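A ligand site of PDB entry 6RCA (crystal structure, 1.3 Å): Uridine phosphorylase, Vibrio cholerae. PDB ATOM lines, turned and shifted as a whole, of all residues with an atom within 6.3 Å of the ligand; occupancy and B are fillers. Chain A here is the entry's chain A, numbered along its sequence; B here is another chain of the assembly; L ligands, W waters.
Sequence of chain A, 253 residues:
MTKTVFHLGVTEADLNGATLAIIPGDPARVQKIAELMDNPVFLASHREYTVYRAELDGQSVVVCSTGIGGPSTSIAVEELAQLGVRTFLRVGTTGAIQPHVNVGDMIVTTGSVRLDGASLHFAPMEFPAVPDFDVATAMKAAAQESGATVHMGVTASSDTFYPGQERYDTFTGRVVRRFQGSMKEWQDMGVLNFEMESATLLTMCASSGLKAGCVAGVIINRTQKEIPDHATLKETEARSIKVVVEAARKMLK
The side-chain carboxylate of Glu 197 sits at hydrogen-bond distance from an oxygen (O1) of the ligand, 2.6 Å away. An oxygen (O5) of the ligand lies within hydrogen-bond range of a ring nitrogen (NE2) of His 7 of chain B, 2.7 Å away. The side-chain amide oxygen of Gln 165 lies close to an oxygen (O3) of the ligand (2.9 Å). The backbone NH (N) of Met 196 lies close to an oxygen (O2) of the ligand (3.4 Å). The guanidinium group (NH2) of Arg 47 of chain B lies within hydrogen-bond range of an oxygen (O4) of the ligand (3.5 Å).
N of Glu 197 is in hydrogen-bond range of OE2 of Glu 195 (2.9 Å). The side-chain carboxylate of Glu 197 lies within salt-bridge range of the guanidinium group of Arg 90 (3.1 Å). The side-chain carboxylate (OE2) of Glu 197 lies within hydrogen-bond range of the backbone NH (N) of Gly 69 (2.8 Å). OE1 of Gln 165 sits at hydrogen-bond distance from NH1 of Arg 167, 3.3 Å away. N of Phe 194 is in hydrogen-bond range of O of Gly 95. O of Phe 194 is in hydrogen-bond range of OG1 of Thr 94, 2.7 Å away. NE of Arg 167 is in hydrogen-bond range of O of Phe 161 (2.9 Å). The backbone carbonyl oxygen (O) of Thr 94 is in hydrogen-bond range of the backbone NH (N) of Ile 219 (3.0 Å).
The backbone carbonyl oxygen (O) of Thr 93 sits close to a nitrogen (N2) of the ligand, at 3.4 Å. Merely in contact with the ligand: Glu 195 (3.6 Å), Ile 68 (3.6 Å), Gly 95 (3.6 Å), Phe 194 (3.6 Å), Phe 161 (3.6 Å), Thr 94 (3.9 Å) and Arg 167 (3.9 Å). Hydrophobic or aromatic side chains within 4 Å of the ligand: Ile 68, Phe 161, Met 196 and His 7 of chain B. 13 residues have an atom within 4 Å of the ligand: Ile 68, Thr 93, Thr 94, Gly 95, Phe 161, Gln 165, Arg 167, Phe 194, Glu 195, Met 196, Glu 197, His 7 of chain B and Arg 47 of chain B.
Water W6 bridges O3 of the ligand and NH1 of Arg 167. Water W4 lies within hydrogen-bond range of O1 of the ligand (2.7 Å), NH1 of Arg 47 of chain B (2.8 Å) and NH2 of Arg 90 (3.4 Å). Water W5 lies within hydrogen-bond range of an oxygen (O5) of the ligand and the guanidinium group of Arg 47 of chain B. Water W1 bridges NH2 of Arg 90 (3.3 Å) and N of Thr 93 (3.4 Å). Water W3 lies within hydrogen-bond range of the side-chain amide oxygen (OE1) of Gln 165, the guanidinium group (NH2) of Arg 222, the guanidinium group (NH1) of Arg 167 and an oxygen (O3) of the ligand.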
ATOM      1  N   GLY A  25       7.097  18.943  -8.177  1.00  0.00           N
ATOM      2  CA  GLY A  25       6.238  19.869  -7.441  1.00  0.00           C
ATOM      3  C   GLY A  25       4.780  19.436  -7.385  1.00  0.00           C
ATOM      4  O   GLY A  25       4.133  19.646  -6.336  1.00  0.00           O
ATOM      5  N   GLY A  67       4.880  20.322  -3.505  1.00  0.00           N
ATOM      6  CA  GLY A  67       4.210  21.603  -3.579  1.00  0.00           C
ATOM      7  C   GLY A  67       5.084  22.688  -4.153  1.00  0.00           C
ATOM      8  O   GLY A  67       6.271  22.459  -4.483  1.00  0.00           O
ATOM      9  N   ILE A  68       4.527  23.876  -4.285  1.00  0.00           N
ATOM     10  CA  ILE A  68       5.256  25.058  -4.763  1.00  0.00           C
ATOM     11  C   ILE A  68       5.999  25.682  -3.600  1.00  0.00           C
ATOM     12  O   ILE A  68       5.382  25.976  -2.553  1.00  0.00           O
ATOM     13  CB  ILE A  68       4.308  26.067  -5.419  1.00  0.00           C
ATOM     14  CG1 ILE A  68       3.699  25.461  -6.696  1.00  0.00           C
ATOM     15  CG2 ILE A  68       5.053  27.390  -5.696  1.00  0.00           C
ATOM     16  CD1 ILE A  68       2.666  26.284  -7.352  1.00  0.00           C
ATOM     17  N   GLY A  69       7.284  25.953  -3.824  1.00  0.00           N
ATOM     18  CA  GLY A  69       8.089  26.779  -2.941  1.00  0.00           C
ATOM     19  C   GLY A  69       9.000  26.018  -2.009  1.00  0.00           C
ATOM     20  O   GLY A  69       8.804  24.845  -1.646  1.00  0.00           O
ATOM     21  N   ARG A  90      15.226  16.493  -8.229  1.00  0.00           N
ATOM     22  CA  ARG A  90      14.127  17.328  -8.610  1.00  0.00           C
ATOM     23  C   ARG A  90      13.927  17.492 -10.100  1.00  0.00           C
ATOM     24  O   ARG A  90      14.859  17.700 -10.794  1.00  0.00           O
ATOM     25  CB  ARG A  90      14.288  18.735  -7.990  1.00  0.00           C
ATOM     26  CG  ARG A  90      13.275  19.732  -8.548  1.00  0.00           C
ATOM     27  CD  ARG A  90      12.342  20.142  -7.553  1.00  0.00           C
ATOM     28  NE  ARG A  90      11.392  21.139  -7.956  1.00  0.00           N
ATOM     29  CZ  ARG A  90      10.210  21.133  -7.425  1.00  0.00           C
ATOM     30  NH1 ARG A  90       9.880  20.174  -6.605  1.00  0.00           N
ATOM     31  NH2 ARG A  90       9.390  22.094  -7.729  1.00  0.00           N
ATOM     32  N   GLY A  92      11.166  19.422 -12.886  1.00  0.00           N
ATOM     33  CA  GLY A  92      10.076  20.406 -12.960  1.00  0.00           C
ATOM     34  C   GLY A  92      10.091  21.150 -14.250  1.00  0.00           C
ATOM     35  O   GLY A  92      10.719  20.660 -15.258  1.00  0.00           O
ATOM     36  N   THR A  93       9.365  22.272 -14.227  1.00  0.00           N
ATOM     37  CA  THR A  93       9.227  23.237 -15.325  1.00  0.00           C
ATOM     38  C   THR A  93       9.876  24.529 -14.976  1.00  0.00           C
ATOM     39  O   THR A  93      10.023  24.883 -13.768  1.00  0.00           O
ATOM     40  CB  THR A  93       7.745  23.467 -15.675  1.00  0.00           C
ATOM     41  OG1 THR A  93       7.073  24.051 -14.516  1.00  0.00           O
ATOM     42  CG2 THR A  93       7.029  22.189 -16.130  1.00  0.00           C
ATOM     43  N   THR A  94      10.239  25.274 -16.010  1.00  0.00           N
ATOM     44  CA  THR A  94      10.973  26.534 -15.795  1.00  0.00           C
ATOM     45  C   THR A  94      10.669  27.506 -16.938  1.00  0.00           C
ATOM     46  O   THR A  94      10.354  27.101 -18.057  1.00  0.00           O
ATOM     47  CB  THR A  94      12.436  26.235 -15.610  1.00  0.00           C
ATOM     48  OG1 THR A  94      13.048  27.450 -15.239  1.00  0.00           O
ATOM     49  CG2 THR A  94      13.112  25.817 -16.881  1.00  0.00           C
ATOM     50  N   GLY A  95      10.820  28.801 -16.613  1.00  0.00           N
ATOM     51  CA  GLY A  95      10.780  29.885 -17.574  1.00  0.00           C
ATOM     52  C   GLY A  95      12.221  30.319 -17.871  1.00  0.00           C
ATOM     53  O   GLY A  95      12.920  30.757 -16.931  1.00  0.00           O
ATOM     54  N   PHE A 161       6.234  33.922  -7.628  1.00  0.00           N
ATOM     55  CA  PHE A 161       6.063  33.804  -9.068  1.00  0.00           C
ATOM     56  C   PHE A 161       6.036  35.128  -9.736  1.00  0.00           C
ATOM     57  O   PHE A 161       6.373  35.266 -10.920  1.00  0.00           O
ATOM     58  CB  PHE A 161       4.838  32.937  -9.346  1.00  0.00           C
ATOM     59  CG  PHE A 161       4.566  32.622 -10.789  1.00  0.00           C
ATOM     60  CD1 PHE A 161       5.215  31.542 -11.355  1.00  0.00           C
ATOM     61  CD2 PHE A 161       3.760  33.379 -11.593  1.00  0.00           C
ATOM     62  CE1 PHE A 161       5.023  31.207 -12.674  1.00  0.00           C
ATOM     63  CE2 PHE A 161       3.491  32.997 -12.907  1.00  0.00           C
ATOM     64  CZ  PHE A 161       4.183  31.921 -13.459  1.00  0.00           C
ATOM     65  N   GLN A 165       9.977  37.436  -9.905  1.00  0.00           N
ATOM     66  CA  GLN A 165      10.321  37.157 -11.319  1.00  0.00           C
ATOM     67  C   GLN A 165      10.130  38.416 -12.156  1.00  0.00           C
ATOM     68  O   GLN A 165      10.081  38.327 -13.390  1.00  0.00           O
ATOM     69  CB  GLN A 165       9.539  35.938 -11.828  1.00  0.00           C
ATOM     70  CG  GLN A 165       9.770  34.692 -11.007  1.00  0.00           C
ATOM     71  CD  GLN A 165       9.290  33.394 -11.621  1.00  0.00           C
ATOM     72  OE1 GLN A 165       9.026  33.329 -12.787  1.00  0.00           O
ATOM     73  NE2 GLN A 165       9.191  32.337 -10.824  1.00  0.00           N
ATOM     74  N   ARG A 167       7.520  40.315 -12.692  1.00  0.00           N
ATOM     75  CA  ARG A 167       6.283  40.417 -13.484  1.00  0.00           C
ATOM     76  C   ARG A 167       5.529  41.673 -13.066  1.00  0.00           C
ATOM     77  O   ARG A 167       5.286  41.859 -11.892  1.00  0.00           O
ATOM     78  CB  ARG A 167       5.417  39.184 -13.271  1.00  0.00           C
ATOM     79  CG  ARG A 167       6.107  37.901 -13.713  1.00  0.00           C
ATOM     80  CD  ARG A 167       5.173  36.736 -13.583  1.00  0.00           C
ATOM     81  NE  ARG A 167       5.893  35.513 -13.808  1.00  0.00           N
ATOM     82  CZ  ARG A 167       5.858  34.767 -14.877  1.00  0.00           C
ATOM     83  NH1 ARG A 167       6.573  33.649 -14.931  1.00  0.00           N
ATOM     84  NH2 ARG A 167       5.089  35.095 -15.892  1.00  0.00           N
ATOM     85  N   PHE A 194      14.202  31.015 -14.352  1.00  0.00           N
ATOM     86  CA  PHE A 194      13.552  31.178 -13.047  1.00  0.00           C
ATOM     87  C   PHE A 194      12.827  29.892 -12.639  1.00  0.00           C
ATOM     88  O   PHE A 194      12.174  29.250 -13.482  1.00  0.00           O
ATOM     89  CB  PHE A 194      12.468  32.244 -13.105  1.00  0.00           C
ATOM     90  CG  PHE A 194      12.951  33.672 -12.963  1.00  0.00           C
ATOM     91  CD1 PHE A 194      13.495  34.136 -11.787  1.00  0.00           C
ATOM     92  CD2 PHE A 194      12.680  34.604 -13.982  1.00  0.00           C
ATOM     93  CE1 PHE A 194      13.893  35.493 -11.654  1.00  0.00           C
ATOM     94  CE2 PHE A 194      13.052  35.946 -13.852  1.00  0.00           C
ATOM     95  CZ  PHE A 194      13.674  36.364 -12.679  1.00  0.00           C
ATOM     96  N   GLU A 195      12.867  29.572 -11.366  1.00  0.00           N
ATOM     97  CA  GLU A 195      11.936  28.658 -10.723  1.00  0.00           C
ATOM     98  C   GLU A 195      11.828  29.023  -9.259  1.00  0.00           C
ATOM     99  O   GLU A 195      12.203  30.143  -8.894  1.00  0.00           O
ATOM    100  CB  GLU A 195      12.207  27.190 -11.066  1.00  0.00           C
ATOM    101  CG  GLU A 195      13.603  26.765 -10.760  1.00  0.00           C
ATOM    102  CD  GLU A 195      13.925  26.620  -9.292  1.00  0.00           C
ATOM    103  OE1 GLU A 195      14.548  27.579  -8.762  1.00  0.00           O
ATOM    104  OE2 GLU A 195      13.445  25.684  -8.624  1.00  0.00           O
ATOM    105  N   MET A 196      11.256  28.140  -8.417  1.00  0.00           N
ATOM    106  CA  MET A 196      10.893  28.573  -7.054  1.00  0.00           C
ATOM    107  C   MET A 196      11.345  27.617  -5.944  1.00  0.00           C
ATOM    108  O   MET A 196      10.918  27.814  -4.782  1.00  0.00           O
ATOM    109  CB  MET A 196       9.378  28.793  -7.005  1.00  0.00           C
ATOM    110  CG  MET A 196       8.890  29.858  -7.907  1.00  0.00           C
ATOM    111  SD  MET A 196       7.095  30.161  -7.843  1.00  0.00           S
ATOM    112  CE  MET A 196       6.887  30.637  -6.139  1.00  0.00           C
ATOM    113  N   GLU A 197      12.164  26.600  -6.197  1.00  0.00           N
ATOM    114  CA  GLU A 197      12.465  25.601  -5.182  1.00  0.00           C
ATOM    115  C   GLU A 197      13.939  25.244  -5.076  1.00  0.00           C
ATOM    116  O   GLU A 197      14.351  24.744  -4.046  1.00  0.00           O
ATOM    117  CB  GLU A 197      11.702  24.291  -5.485  1.00  0.00           C
ATOM    118  CG  GLU A 197      10.203  24.460  -5.399  1.00  0.00           C
ATOM    119  CD  GLU A 197       9.492  25.068  -6.578  1.00  0.00           C
ATOM    120  OE1 GLU A 197      10.042  25.143  -7.718  1.00  0.00           O
ATOM    121  OE2 GLU A 197       8.319  25.459  -6.417  1.00  0.00           O
ATOM    122  N   ILE A 219       9.354  25.629 -20.464  1.00  0.00           N
ATOM    123  CA  ILE A 219       7.953  25.731 -20.911  1.00  0.00           C
ATOM    124  C   ILE A 219       7.606  27.103 -21.453  1.00  0.00           C
ATOM    125  O   ILE A 219       6.552  27.239 -22.078  1.00  0.00           O
ATOM    126  CB  ILE A 219       6.973  25.271 -19.802  1.00  0.00           C
ATOM    127  CG1 ILE A 219       6.970  26.193 -18.566  1.00  0.00           C
ATOM    128  CG2 ILE A 219       7.234  23.850 -19.465  1.00  0.00           C
ATOM    129  CD1 ILE A 219       5.789  25.958 -17.656  1.00  0.00           C
ATOM    130  N   ILE A 220       8.459  28.095 -21.216  1.00  0.00           N
ATOM    131  CA  ILE A 220       8.212  29.460 -21.667  1.00  0.00           C
ATOM    132  C   ILE A 220       9.542  30.170 -21.711  1.00  0.00           C
ATOM    133  O   ILE A 220      10.435  29.774 -20.964  1.00  0.00           O
ATOM    134  CB  ILE A 220       7.202  30.182 -20.776  1.00  0.00           C
ATOM    135  CG1 ILE A 220       6.559  31.331 -21.540  1.00  0.00           C
ATOM    136  CG2 ILE A 220       7.776  30.554 -19.471  1.00  0.00           C
ATOM    137  CD1 ILE A 220       5.328  30.903 -22.179  1.00  0.00           C
ATOM    138  N   ARG A 222      10.756  34.144 -21.372  1.00  0.00           N
ATOM    139  CA  ARG A 222      10.281  35.487 -21.041  1.00  0.00           C
ATOM    140  C   ARG A 222      10.636  36.495 -22.120  1.00  0.00           C
ATOM    141  O   ARG A 222      10.064  37.584 -22.103  1.00  0.00           O
ATOM    142  CB  ARG A 222      10.870  35.902 -19.687  1.00  0.00           C
ATOM    143  CG  ARG A 222      10.337  35.147 -18.474  1.00  0.00           C
ATOM    144  CD  ARG A 222       8.901  35.503 -18.133  1.00  0.00           C
ATOM    145  NE  ARG A 222       8.746  36.897 -17.677  1.00  0.00           N
ATOM    146  CZ  ARG A 222       9.079  37.349 -16.458  1.00  0.00           C
ATOM    147  NH1 ARG A 222       8.989  38.657 -16.178  1.00  0.00           N
ATOM    148  NH2 ARG A 222       9.464  36.500 -15.541  1.00  0.00           N
ATOM    149  N   HIS B   7      -2.620  29.744 -12.221  1.00  0.00           N
ATOM    150  CA  HIS B   7      -2.583  28.568 -11.332  1.00  0.00           C
ATOM    151  C   HIS B   7      -3.947  28.106 -10.854  1.00  0.00           C
ATOM    152  O   HIS B   7      -4.150  26.899 -10.734  1.00  0.00           O
ATOM    153  CB  HIS B   7      -1.694  28.816 -10.105  1.00  0.00           C
ATOM    154  CG  HIS B   7      -0.268  29.075 -10.441  1.00  0.00           C
ATOM    155  ND1 HIS B   7       0.188  30.329 -10.815  1.00  0.00           N
ATOM    156  CD2 HIS B   7       0.828  28.274 -10.482  1.00  0.00           C
ATOM    157  CE1 HIS B   7       1.507  30.249 -11.048  1.00  0.00           C
ATOM    158  NE2 HIS B   7       1.920  29.002 -10.901  1.00  0.00           N
ATOM    159  N   ARG B  47      -2.854  21.326  -8.337  1.00  0.00           N
ATOM    160  CA  ARG B  47      -1.760  21.418  -7.385  1.00  0.00           C
ATOM    161  C   ARG B  47      -2.378  21.529  -5.977  1.00  0.00           C
ATOM    162  O   ARG B  47      -3.384  20.843  -5.704  1.00  0.00           O
ATOM    163  CB  ARG B  47      -0.826  22.577  -7.767  1.00  0.00           C
ATOM    164  CG  ARG B  47      -0.034  22.336  -9.054  1.00  0.00           C
ATOM    165  CD  ARG B  47       0.854  23.510  -9.337  1.00  0.00           C
ATOM    166  NE  ARG B  47       1.739  23.421 -10.425  1.00  0.00           N
ATOM    167  CZ  ARG B  47       3.049  23.102 -10.345  1.00  0.00           C
ATOM    168  NH1 ARG B  47       3.602  22.698  -9.218  1.00  0.00           N
ATOM    169  NH2 ARG B  47       3.820  23.191 -11.418  1.00  0.00           N
ATOM    170  N   ILE B  75       0.950  33.180  -4.505  1.00  0.00           N
ATOM    171  CA  ILE B  75       0.329  32.956  -5.809  1.00  0.00           C
ATOM    172  C   ILE B  75      -1.217  33.008  -5.701  1.00  0.00           C
ATOM    173  O   ILE B  75      -1.878  33.686  -6.502  1.00  0.00           O
ATOM    174  CB  ILE B  75       0.777  31.602  -6.425  1.00  0.00           C
ATOM    175  CG1 ILE B  75       2.248  31.659  -6.858  1.00  0.00           C
ATOM    176  CG2 ILE B  75      -0.166  31.147  -7.515  1.00  0.00           C
ATOM    177  CD1 ILE B  75       2.849  30.325  -7.196  1.00  0.00           C
HETATM  178  O1  LIG L   1       6.808  25.270  -8.473  1.00  0.00           O
HETATM  179  C1  LIG L   1       6.861  26.457  -9.282  1.00  0.00           C
HETATM  180  C2  LIG L   1       8.085  26.363 -10.201  1.00  0.00           C
HETATM  181  O2  LIG L   1       8.522  27.693 -10.433  1.00  0.00           O
HETATM  182  C3  LIG L   1       8.401  28.082 -11.698  1.00  0.00           C
HETATM  183  N1  LIG L   1       8.724  29.321 -12.167  1.00  0.00           N
HETATM  184  C4  LIG L   1       8.520  29.572 -13.499  1.00  0.00           C
HETATM  185  O3  LIG L   1       8.881  30.666 -13.928  1.00  0.00           O
HETATM  186  C5  LIG L   1       7.986  28.639 -14.398  1.00  0.00           C
HETATM  187  C6  LIG L   1       7.580  27.290 -13.841  1.00  0.00           C
HETATM  188  N2  LIG L   1       7.861  27.113 -12.457  1.00  0.00           N
HETATM  189  C7  LIG L   1       7.573  25.946 -11.591  1.00  0.00           C
HETATM  190  O4  LIG L   1       6.178  25.739 -11.478  1.00  0.00           O
HETATM  191  C8  LIG L   1       5.680  26.467 -10.337  1.00  0.00           C
HETATM  192  C9  LIG L   1       5.198  27.910 -10.643  1.00  0.00           C
HETATM  193  O5  LIG L   1       4.196  27.800 -11.670  1.00  0.00           O
HETATM  194  O   HOH W   1       8.965  22.919 -10.929  1.00  0.00           O
HETATM  195  O   HOH W   2       4.422  28.036 -14.539  1.00  0.00           O
HETATM  196  O   HOH W   3       9.800  33.636 -15.535  1.00  0.00           O
HETATM  197  O   HOH W   4       6.405  22.732  -9.145  1.00  0.00           O
HETATM  198  O   HOH W   5       3.103  25.511 -12.839  1.00  0.00           O
HETATM  199  O   HOH W   6       7.900  31.470 -16.209  1.00  0.00           O
